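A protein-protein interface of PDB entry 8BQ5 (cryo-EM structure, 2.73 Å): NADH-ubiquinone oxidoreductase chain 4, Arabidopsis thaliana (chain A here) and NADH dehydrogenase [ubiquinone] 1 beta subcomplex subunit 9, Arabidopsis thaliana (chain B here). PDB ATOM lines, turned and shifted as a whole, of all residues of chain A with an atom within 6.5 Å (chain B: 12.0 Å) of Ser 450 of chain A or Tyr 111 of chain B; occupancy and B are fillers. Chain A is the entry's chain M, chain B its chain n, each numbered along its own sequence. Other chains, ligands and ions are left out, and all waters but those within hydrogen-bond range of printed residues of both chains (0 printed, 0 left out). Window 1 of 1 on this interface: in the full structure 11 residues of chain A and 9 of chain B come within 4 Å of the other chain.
Of the 12 printed residues of chain B, 6 touch a printed residue of chain A. Hydrophobic or aromatic side chains of chain B that line the printed part of chain A: Val 108 and Tyr 111. Along chain B the printed residues that touch a printed residue of chain A span positions 106 to 113. Among the printed residues, no Asp or Glu carboxylate lies within 4 Å of a Lys or Arg side-chain nitrogen of the other chain.
OG of Ser 110 of chain A sits at hydrogen-bond distance from NH2 of Arg 455 of chain A, at 2.6 Å. The backbone carbonyl oxygen of Val 354 of chain A is in hydrogen-bond range of the guanidinium group of Arg 358 of chain A (3.2 Å). NE of Arg 358 of chain A lies within hydrogen-bond range of O of Ser 450 of chain A (2.8 Å). The side-chain carboxylate (OE1) of Glu 456 of chain A is in salt-bridge range of the guanidinium group (NH2) of Arg 358 of chain A (2.8 Å). The backbone NH of Arg 455 of chain A sits close to the side-chain amide oxygen of Asn 453 of chain A, at 3.3 Å. The backbone NH (N) of Glu 456 of chain A is in hydrogen-bond range of the side-chain amide oxygen (OD1) of Asn 453 of chain A.
OG of Ser 110 of chain A sits at hydrogen-bond distance from O of Gly 112 of chain B. The backbone carbonyl oxygen (O) of Asp 357 of chain A sits at hydrogen-bond distance from the side-chain hydroxyl (OH) of Tyr 111 of chain B (3.2 Å). O of Glu 106 of chain B is in hydrogen-bond range of N of Phe 449 of chain A. The backbone carbonyl oxygen (O) of Phe 449 of chain A is in hydrogen-bond range of the backbone NH (N) of Val 108 of chain B (2.8 Å). OG of Ser 450 of chain A lies within hydrogen-bond range of O of Val 108 of chain B (2.9 Å). The backbone carbonyl oxygen (O) of Tyr 111 of chain B is in hydrogen-bond range of the side-chain amide nitrogen (ND2) of Asn 453 of chain A (3.1 Å). The guanidinium group (NH2) of Arg 455 of chain A sits at hydrogen-bond distance from the backbone carbonyl oxygen (O) of Gly 112 of chain B (3.2 Å).
Of chain B, only Tyr 111 (3.2 Å) comes within 4 Å of Asp 357 of chain A. No residue of chain B comes within 4 Å of Met 374 of chain A. Phe 449 of chain A touches three residues of chain B. Of chain B, only Val 108 (2.9 Å) and Tyr 111 (3.7 Å) come within 4 Å of Ser 450 of chain A. No residue of chain B comes within 4 Å of Asp 451 of chain A. No residue of chain B comes within 4 Å of Leu 452 of chain A. Of chain B, only Tyr 111 (3.1 Å) and Gly 112 (3.5 Å) come within 4 Å of Asn 453 of chain A. Glu 456 of chain A touches none of the printed residues of chain B. Ile 105 of chain B touches none of the printed residues of chain A. Of chain A, only Asp 357 (3.2 Å), Arg 358 (3.6 Å), Ser 450 (3.7 Å) and Asn 453 (3.1 Å) come within 4 Å of Tyr 111 of chain B. Of the printed residues of chain A, Gly 112 of chain B touches Ser 110, Asn 453 and Arg 455. Printed residues of chain A within 4 Å of Leu 113 of chain B: Ser 110. The nearest residue of chain A that does not touch Tyr 111 of chain B is Glu 456 of chain A (5.1 Å).
Among the printed residues, merely in contact across the chains: Ser 110 of chain A with Leu 113 of chain B (3.6 Å), Arg 358 of chain A with Tyr 111 of chain B (3.6 Å), Lys 448 of chain A with Glu 106 of chain B (2.8 Å), Lys 448 of chain A with Val 108 of chain B (3.5 Å), Phe 449 of chain A with Ile 107 of chain B (3.5 Å), Ser 450 of chain A with Tyr 111 of chain B (3.7 Å) and Asn 453 of chain A with Gly 112 of chain B (3.5 Å).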
ATOM      1  N   SER A 110       9.093 -17.506  27.851  1.00  0.00           N
ATOM      2  CA  SER A 110       7.775 -16.998  27.484  1.00  0.00           C
ATOM      3  C   SER A 110       6.817 -18.129  27.130  1.00  0.00           C
ATOM      4  O   SER A 110       5.609 -18.023  27.373  1.00  0.00           O
ATOM      5  CB  SER A 110       7.901 -16.012  26.324  1.00  0.00           C
ATOM      6  OG  SER A 110       8.594 -14.847  26.732  1.00  0.00           O
ATOM      7  N   VAL A 354      15.583 -15.761  17.927  1.00  0.00           N
ATOM      8  CA  VAL A 354      14.847 -14.515  18.117  1.00  0.00           C
ATOM      9  C   VAL A 354      14.012 -14.204  16.883  1.00  0.00           C
ATOM     10  O   VAL A 354      12.833 -13.842  16.985  1.00  0.00           O
ATOM     11  CB  VAL A 354      15.824 -13.368  18.442  1.00  0.00           C
ATOM     12  CG1 VAL A 354      15.160 -12.020  18.237  1.00  0.00           C
ATOM     13  CG2 VAL A 354      16.354 -13.495  19.860  1.00  0.00           C
ATOM     14  N   ASP A 357      11.151 -16.894  16.403  1.00  0.00           N
ATOM     15  CA  ASP A 357      10.068 -16.796  17.377  1.00  0.00           C
ATOM     16  C   ASP A 357       9.014 -15.790  16.941  1.00  0.00           C
ATOM     17  O   ASP A 357       7.816 -16.014  17.153  1.00  0.00           O
ATOM     18  CB  ASP A 357      10.621 -16.417  18.750  1.00  0.00           C
ATOM     19  CG  ASP A 357      11.077 -17.619  19.550  1.00  0.00           C
ATOM     20  OD1 ASP A 357      11.222 -17.485  20.782  1.00  0.00           O
ATOM     21  OD2 ASP A 357      11.296 -18.693  18.951  1.00  0.00           O
ATOM     22  N   ARG A 358       9.433 -14.679  16.338  1.00  0.00           N
ATOM     23  CA  ARG A 358       8.510 -13.646  15.889  1.00  0.00           C
ATOM     24  C   ARG A 358       7.858 -13.985  14.552  1.00  0.00           C
ATOM     25  O   ARG A 358       6.646 -13.817  14.394  1.00  0.00           O
ATOM     26  CB  ARG A 358       9.240 -12.302  15.780  1.00  0.00           C
ATOM     27  CG  ARG A 358       9.776 -11.772  17.094  1.00  0.00           C
ATOM     28  CD  ARG A 358      10.994 -10.889  16.880  1.00  0.00           C
ATOM     29  NE  ARG A 358      11.297 -10.074  18.050  1.00  0.00           N
ATOM     30  CZ  ARG A 358      11.791 -10.545  19.187  1.00  0.00           C
ATOM     31  NH1 ARG A 358      12.038 -11.835  19.351  1.00  0.00           N
ATOM     32  NH2 ARG A 358      12.042  -9.703  20.184  1.00  0.00           N
ATOM     33  N   HIS A 359       8.640 -14.468  13.587  1.00  0.00           N
ATOM     34  CA  HIS A 359       8.185 -14.534  12.205  1.00  0.00           C
ATOM     35  C   HIS A 359       7.959 -15.949  11.694  1.00  0.00           C
ATOM     36  O   HIS A 359       7.324 -16.114  10.648  1.00  0.00           O
ATOM     37  CB  HIS A 359       9.188 -13.811  11.303  1.00  0.00           C
ATOM     38  CG  HIS A 359       9.458 -12.405  11.735  1.00  0.00           C
ATOM     39  ND1 HIS A 359       8.448 -11.498  11.969  1.00  0.00           N
ATOM     40  CD2 HIS A 359      10.615 -11.763  12.020  1.00  0.00           C
ATOM     41  CE1 HIS A 359       8.972 -10.348  12.355  1.00  0.00           C
ATOM     42  NE2 HIS A 359      10.285 -10.483  12.395  1.00  0.00           N
ATOM     43  N   LYS A 360       8.459 -16.962  12.402  1.00  0.00           N
ATOM     44  CA  LYS A 360       8.198 -18.363  12.082  1.00  0.00           C
ATOM     45  C   LYS A 360       8.653 -18.717  10.668  1.00  0.00           C
ATOM     46  O   LYS A 360       7.990 -19.458   9.940  1.00  0.00           O
ATOM     47  CB  LYS A 360       6.720 -18.702  12.281  1.00  0.00           C
ATOM     48  CG  LYS A 360       6.295 -18.715  13.734  1.00  0.00           C
ATOM     49  CD  LYS A 360       6.972 -19.849  14.480  1.00  0.00           C
ATOM     50  CE  LYS A 360       7.296 -19.449  15.907  1.00  0.00           C
ATOM     51  NZ  LYS A 360       6.073 -19.097  16.676  1.00  0.00           N
ATOM     52  N   THR A 373      14.379  -1.703  11.466  1.00  0.00           N
ATOM     53  CA  THR A 373      13.332  -2.042  12.417  1.00  0.00           C
ATOM     54  C   THR A 373      13.847  -2.723  13.675  1.00  0.00           C
ATOM     55  O   THR A 373      13.191  -2.629  14.716  1.00  0.00           O
ATOM     56  CB  THR A 373      12.281  -2.948  11.759  1.00  0.00           C
ATOM     57  OG1 THR A 373      12.912  -4.134  11.262  1.00  0.00           O
ATOM     58  CG2 THR A 373      11.602  -2.225  10.613  1.00  0.00           C
ATOM     59  N   MET A 374      14.994  -3.395  13.610  1.00  0.00           N
ATOM     60  CA  MET A 374      15.586  -4.072  14.766  1.00  0.00           C
ATOM     61  C   MET A 374      17.060  -3.699  14.894  1.00  0.00           C
ATOM     62  O   MET A 374      17.942  -4.547  14.744  1.00  0.00           O
ATOM     63  CB  MET A 374      15.420  -5.585  14.641  1.00  0.00           C
ATOM     64  CG  MET A 374      13.999  -6.040  14.364  1.00  0.00           C
ATOM     65  SD  MET A 374      13.886  -7.796  13.976  1.00  0.00           S
ATOM     66  CE  MET A 374      14.205  -8.521  15.580  1.00  0.00           C
ATOM     67  N   PHE A 377      18.943  -5.753  17.734  1.00  0.00           N
ATOM     68  CA  PHE A 377      19.229  -7.103  17.261  1.00  0.00           C
ATOM     69  C   PHE A 377      20.298  -7.080  16.176  1.00  0.00           C
ATOM     70  O   PHE A 377      21.174  -7.951  16.140  1.00  0.00           O
ATOM     71  CB  PHE A 377      17.952  -7.770  16.747  1.00  0.00           C
ATOM     72  CG  PHE A 377      18.205  -8.980  15.892  1.00  0.00           C
ATOM     73  CD1 PHE A 377      18.390 -10.225  16.468  1.00  0.00           C
ATOM     74  CD2 PHE A 377      18.256  -8.872  14.512  1.00  0.00           C
ATOM     75  CE1 PHE A 377      18.628 -11.337  15.685  1.00  0.00           C
ATOM     76  CE2 PHE A 377      18.494  -9.980  13.726  1.00  0.00           C
ATOM     77  CZ  PHE A 377      18.679 -11.214  14.313  1.00  0.00           C
ATOM     78  N   LYS A 448       5.551  -6.351  10.359  1.00  0.00           N
ATOM     79  CA  LYS A 448       5.359  -6.153  11.788  1.00  0.00           C
ATOM     80  C   LYS A 448       6.589  -6.662  12.526  1.00  0.00           C
ATOM     81  O   LYS A 448       6.946  -7.838  12.401  1.00  0.00           O
ATOM     82  CB  LYS A 448       4.109  -6.892  12.262  1.00  0.00           C
ATOM     83  CG  LYS A 448       3.486  -6.341  13.516  1.00  0.00           C
ATOM     84  CD  LYS A 448       1.999  -6.220  13.383  1.00  0.00           C
ATOM     85  CE  LYS A 448       1.272  -7.456  13.848  1.00  0.00           C
ATOM     86  NZ  LYS A 448       1.502  -7.699  15.293  1.00  0.00           N
ATOM     87  N   PHE A 449       7.226  -5.791  13.306  1.00  0.00           N
ATOM     88  CA  PHE A 449       8.512  -6.119  13.904  1.00  0.00           C
ATOM     89  C   PHE A 449       8.571  -5.672  15.358  1.00  0.00           C
ATOM     90  O   PHE A 449       7.796  -4.821  15.801  1.00  0.00           O
ATOM     91  CB  PHE A 449       9.673  -5.487  13.126  1.00  0.00           C
ATOM     92  CG  PHE A 449       9.662  -5.807  11.661  1.00  0.00           C
ATOM     93  CD1 PHE A 449       8.977  -5.002  10.768  1.00  0.00           C
ATOM     94  CD2 PHE A 449      10.323  -6.922  11.180  1.00  0.00           C
ATOM     95  CE1 PHE A 449       8.961  -5.299   9.422  1.00  0.00           C
ATOM     96  CE2 PHE A 449      10.308  -7.226   9.836  1.00  0.00           C
ATOM     97  CZ  PHE A 449       9.627  -6.412   8.955  1.00  0.00           C
ATOM     98  N   SER A 450       9.498  -6.281  16.095  1.00  0.00           N
ATOM     99  CA  SER A 450       9.795  -5.916  17.473  1.00  0.00           C
ATOM    100  C   SER A 450      11.255  -6.226  17.754  1.00  0.00           C
ATOM    101  O   SER A 450      11.698  -7.358  17.546  1.00  0.00           O
ATOM    102  CB  SER A 450       8.903  -6.671  18.464  1.00  0.00           C
ATOM    103  OG  SER A 450       8.999  -6.112  19.761  1.00  0.00           O
ATOM    104  N   ASP A 451      11.993  -5.228  18.234  1.00  0.00           N
ATOM    105  CA  ASP A 451      13.376  -5.439  18.629  1.00  0.00           C
ATOM    106  C   ASP A 451      13.434  -6.293  19.898  1.00  0.00           C
ATOM    107  O   ASP A 451      12.414  -6.732  20.437  1.00  0.00           O
ATOM    108  CB  ASP A 451      14.081  -4.098  18.823  1.00  0.00           C
ATOM    109  CG  ASP A 451      15.532  -4.135  18.403  1.00  0.00           C
ATOM    110  OD1 ASP A 451      16.104  -5.241  18.341  1.00  0.00           O
ATOM    111  OD2 ASP A 451      16.101  -3.058  18.131  1.00  0.00           O
ATOM    112  N   LEU A 452      14.651  -6.535  20.379  1.00  0.00           N
ATOM    113  CA  LEU A 452      14.848  -7.415  21.524  1.00  0.00           C
ATOM    114  C   LEU A 452      14.219  -6.833  22.783  1.00  0.00           C
ATOM    115  O   LEU A 452      14.311  -5.631  23.047  1.00  0.00           O
ATOM    116  CB  LEU A 452      16.337  -7.659  21.764  1.00  0.00           C
ATOM    117  CG  LEU A 452      17.248  -7.919  20.566  1.00  0.00           C
ATOM    118  CD1 LEU A 452      18.684  -7.628  20.949  1.00  0.00           C
ATOM    119  CD2 LEU A 452      17.109  -9.349  20.075  1.00  0.00           C
ATOM    120  N   ASN A 453      13.582  -7.698  23.567  1.00  0.00           N
ATOM    121  CA  ASN A 453      13.016  -7.285  24.840  1.00  0.00           C
ATOM    122  C   ASN A 453      14.086  -7.347  25.928  1.00  0.00           C
ATOM    123  O   ASN A 453      15.259  -7.631  25.672  1.00  0.00           O
ATOM    124  CB  ASN A 453      11.798  -8.140  25.194  1.00  0.00           C
ATOM    125  CG  ASN A 453      12.109  -9.626  25.274  1.00  0.00           C
ATOM    126  OD1 ASN A 453      13.265 -10.036  25.359  1.00  0.00           O
ATOM    127  ND2 ASN A 453      11.065 -10.442  25.262  1.00  0.00           N
ATOM    128  N   GLY A 454      13.666  -7.089  27.167  1.00  0.00           N
ATOM    129  CA  GLY A 454      14.612  -7.070  28.270  1.00  0.00           C
ATOM    130  C   GLY A 454      15.243  -8.420  28.543  1.00  0.00           C
ATOM    131  O   GLY A 454      16.413  -8.502  28.920  1.00  0.00           O
ATOM    132  N   ARG A 455      14.472  -9.495  28.378  1.00  0.00           N
ATOM    133  CA  ARG A 455      15.015 -10.828  28.612  1.00  0.00           C
ATOM    134  C   ARG A 455      16.016 -11.210  27.534  1.00  0.00           C
ATOM    135  O   ARG A 455      17.063 -11.798  27.826  1.00  0.00           O
ATOM    136  CB  ARG A 455      13.886 -11.853  28.680  1.00  0.00           C
ATOM    137  CG  ARG A 455      14.323 -13.213  29.185  1.00  0.00           C
ATOM    138  CD  ARG A 455      13.143 -14.162  29.302  1.00  0.00           C
ATOM    139  NE  ARG A 455      12.091 -13.845  28.343  1.00  0.00           N
ATOM    140  CZ  ARG A 455      12.007 -14.367  27.128  1.00  0.00           C
ATOM    141  NH1 ARG A 455      12.881 -15.261  26.697  1.00  0.00           N
ATOM    142  NH2 ARG A 455      11.018 -13.983  26.325  1.00  0.00           N
ATOM    143  N   GLU A 456      15.707 -10.888  26.279  1.00  0.00           N
ATOM    144  CA  GLU A 456      16.609 -11.219  25.185  1.00  0.00           C
ATOM    145  C   GLU A 456      17.906 -10.427  25.281  1.00  0.00           C
ATOM    146  O   GLU A 456      18.976 -10.941  24.940  1.00  0.00           O
ATOM    147  CB  GLU A 456      15.913 -10.973  23.848  1.00  0.00           C
ATOM    148  CG  GLU A 456      14.944 -12.079  23.464  1.00  0.00           C
ATOM    149  CD  GLU A 456      13.816 -11.600  22.573  1.00  0.00           C
ATOM    150  OE1 GLU A 456      13.639 -10.371  22.438  1.00  0.00           O
ATOM    151  OE2 GLU A 456      13.105 -12.455  22.007  1.00  0.00           O
ATOM    152  N   GLY B 104       2.923   1.125   5.887  1.00  0.00           N
ATOM    153  CA  GLY B 104       2.401  -0.148   6.335  1.00  0.00           C
ATOM    154  C   GLY B 104       3.298  -0.916   7.274  1.00  0.00           C
ATOM    155  O   GLY B 104       3.153  -2.138   7.382  1.00  0.00           O
ATOM    156  N   ILE B 105       4.223  -0.247   7.956  1.00  0.00           N
ATOM    157  CA  ILE B 105       5.137  -0.896   8.886  1.00  0.00           C
ATOM    158  C   ILE B 105       4.645  -0.623  10.299  1.00  0.00           C
ATOM    159  O   ILE B 105       4.341   0.522  10.651  1.00  0.00           O
ATOM    160  CB  ILE B 105       6.580  -0.404   8.700  1.00  0.00           C
ATOM    161  CG1 ILE B 105       7.072  -0.699   7.282  1.00  0.00           C
ATOM    162  CG2 ILE B 105       7.499  -1.055   9.726  1.00  0.00           C
ATOM    163  CD1 ILE B 105       6.823  -2.111   6.823  1.00  0.00           C
ATOM    164  N   GLU B 106       4.561  -1.672  11.107  1.00  0.00           N
ATOM    165  CA  GLU B 106       4.120  -1.571  12.487  1.00  0.00           C
ATOM    166  C   GLU B 106       5.223  -2.045  13.420  1.00  0.00           C
ATOM    167  O   GLU B 106       5.925  -3.018  13.126  1.00  0.00           O
ATOM    168  CB  GLU B 106       2.839  -2.378  12.706  1.00  0.00           C
ATOM    169  CG  GLU B 106       2.064  -2.599  11.423  1.00  0.00           C
ATOM    170  CD  GLU B 106       0.708  -3.227  11.640  1.00  0.00           C
ATOM    171  OE1 GLU B 106       0.618  -4.460  11.711  1.00  0.00           O
ATOM    172  OE2 GLU B 106      -0.289  -2.491  11.729  1.00  0.00           O
ATOM    173  N   ILE B 107       5.388  -1.337  14.531  1.00  0.00           N
ATOM    174  CA  ILE B 107       6.362  -1.677  15.559  1.00  0.00           C
ATOM    175  C   ILE B 107       5.594  -2.120  16.797  1.00  0.00           C
ATOM    176  O   ILE B 107       4.772  -1.363  17.327  1.00  0.00           O
ATOM    177  CB  ILE B 107       7.283  -0.486  15.877  1.00  0.00           C
ATOM    178  CG1 ILE B 107       7.985   0.013  14.611  1.00  0.00           C
ATOM    179  CG2 ILE B 107       8.300  -0.868  16.937  1.00  0.00           C
ATOM    180  CD1 ILE B 107       8.718  -1.058  13.838  1.00  0.00           C
ATOM    181  N   VAL B 108       5.859  -3.342  17.253  1.00  0.00           N
ATOM    182  CA  VAL B 108       5.164  -3.930  18.394  1.00  0.00           C
ATOM    183  C   VAL B 108       5.956  -3.654  19.659  1.00  0.00           C
ATOM    184  O   VAL B 108       7.182  -3.825  19.692  1.00  0.00           O
ATOM    185  CB  VAL B 108       4.954  -5.444  18.208  1.00  0.00           C
ATOM    186  CG1 VAL B 108       4.088  -5.998  19.328  1.00  0.00           C
ATOM    187  CG2 VAL B 108       4.327  -5.729  16.865  1.00  0.00           C
ATOM    188  N   TYR B 109       5.259  -3.227  20.704  1.00  0.00           N
ATOM    189  CA  TYR B 109       5.844  -3.075  22.025  1.00  0.00           C
ATOM    190  C   TYR B 109       5.401  -4.237  22.904  1.00  0.00           C
ATOM    191  O   TYR B 109       4.447  -4.948  22.579  1.00  0.00           O
ATOM    192  CB  TYR B 109       5.424  -1.752  22.665  1.00  0.00           C
ATOM    193  CG  TYR B 109       5.932  -0.528  21.948  1.00  0.00           C
ATOM    194  CD1 TYR B 109       7.164  -0.529  21.308  1.00  0.00           C
ATOM    195  CD2 TYR B 109       5.175   0.632  21.908  1.00  0.00           C
ATOM    196  CE1 TYR B 109       7.625   0.594  20.653  1.00  0.00           C
ATOM    197  CE2 TYR B 109       5.625   1.756  21.259  1.00  0.00           C
ATOM    198  CZ  TYR B 109       6.849   1.734  20.632  1.00  0.00           C
ATOM    199  OH  TYR B 109       7.296   2.860  19.984  1.00  0.00           O
ATOM    200  N   ASN B 110       6.110  -4.424  24.017  1.00  0.00           N
ATOM    201  CA  ASN B 110       5.737  -5.408  25.037  1.00  0.00           C
ATOM    202  C   ASN B 110       5.594  -6.814  24.459  1.00  0.00           C
ATOM    203  O   ASN B 110       4.634  -7.530  24.753  1.00  0.00           O
ATOM    204  CB  ASN B 110       4.451  -4.991  25.755  1.00  0.00           C
ATOM    205  CG  ASN B 110       4.523  -3.588  26.311  1.00  0.00           C
ATOM    206  OD1 ASN B 110       5.408  -3.268  27.107  1.00  0.00           O
ATOM    207  ND2 ASN B 110       3.587  -2.743  25.902  1.00  0.00           N
ATOM    208  N   TYR B 111       6.550  -7.219  23.629  1.00  0.00           N
ATOM    209  CA  TYR B 111       6.542  -8.570  23.094  1.00  0.00           C
ATOM    210  C   TYR B 111       7.384  -9.495  23.967  1.00  0.00           C
ATOM    211  O   TYR B 111       8.382  -9.084  24.564  1.00  0.00           O
ATOM    212  CB  TYR B 111       7.067  -8.589  21.658  1.00  0.00           C
ATOM    213  CG  TYR B 111       7.082  -9.969  21.044  1.00  0.00           C
ATOM    214  CD1 TYR B 111       5.908 -10.564  20.606  1.00  0.00           C
ATOM    215  CD2 TYR B 111       8.265 -10.684  20.922  1.00  0.00           C
ATOM    216  CE1 TYR B 111       5.912 -11.827  20.052  1.00  0.00           C
ATOM    217  CE2 TYR B 111       8.278 -11.950  20.370  1.00  0.00           C
ATOM    218  CZ  TYR B 111       7.099 -12.516  19.938  1.00  0.00           C
ATOM    219  OH  TYR B 111       7.100 -13.776  19.387  1.00  0.00           O
ATOM    220  N   GLY B 112       6.966 -10.755  24.040  1.00  0.00           N
ATOM    221  CA  GLY B 112       7.728 -11.750  24.770  1.00  0.00           C
ATOM    222  C   GLY B 112       7.601 -11.674  26.274  1.00  0.00           C
ATOM    223  O   GLY B 112       8.506 -12.121  26.987  1.00  0.00           O
ATOM    224  N   LEU B 113       6.509 -11.106  26.779  1.00  0.00           N
ATOM    225  CA  LEU B 113       6.278 -11.058  28.214  1.00  0.00           C
ATOM    226  C   LEU B 113       6.030 -12.456  28.769  1.00  0.00           C
ATOM    227  O   LEU B 113       5.554 -13.354  28.069  1.00  0.00           O
ATOM    228  CB  LEU B 113       5.088 -10.155  28.536  1.00  0.00           C
ATOM    229  CG  LEU B 113       5.284  -8.662  28.277  1.00  0.00           C
ATOM    230  CD1 LEU B 113       3.963  -7.925  28.400  1.00  0.00           C
ATOM    231  CD2 LEU B 113       6.302  -8.098  29.251  1.00  0.00           C
ATOM    232  N   GLU B 114       6.362 -12.635  30.050  1.00  0.00           N
ATOM    233  CA  GLU B 114       6.228 -13.950  30.666  1.00  0.00           C
ATOM    234  C   GLU B 114       4.769 -14.356  30.844  1.00  0.00           C
ATOM    235  O   GLU B 114       4.456 -15.551  30.819  1.00  0.00           O
ATOM    236  CB  GLU B 114       6.976 -13.984  32.002  1.00  0.00           C
ATOM    237  CG  GLU B 114       6.727 -12.791  32.908  1.00  0.00           C
ATOM    238  CD  GLU B 114       7.289 -12.989  34.306  1.00  0.00           C
ATOM    239  OE1 GLU B 114       8.179 -13.849  34.480  1.00  0.00           O
ATOM    240  OE2 GLU B 114       6.846 -12.280  35.231  1.00  0.00           O
ATOM    241  N   ASP B 115       3.865 -13.396  31.016  1.00  0.00           N
ATOM    242  CA  ASP B 115       2.444 -13.723  31.117  1.00  0.00           C
ATOM    243  C   ASP B 115       1.808 -13.825  29.735  1.00  0.00           C
ATOM    244  O   ASP B 115       0.636 -13.500  29.555  1.00  0.00           O
ATOM    245  CB  ASP B 115       1.694 -12.687  31.958  1.00  0.00           C
ATOM    246  CG  ASP B 115       1.999 -12.806  33.438  1.00  0.00           C
ATOM    247  OD1 ASP B 115       2.615 -13.815  33.840  1.00  0.00           O
ATOM    248  OD2 ASP B 115       1.605 -11.900  34.202  1.00  0.00           O
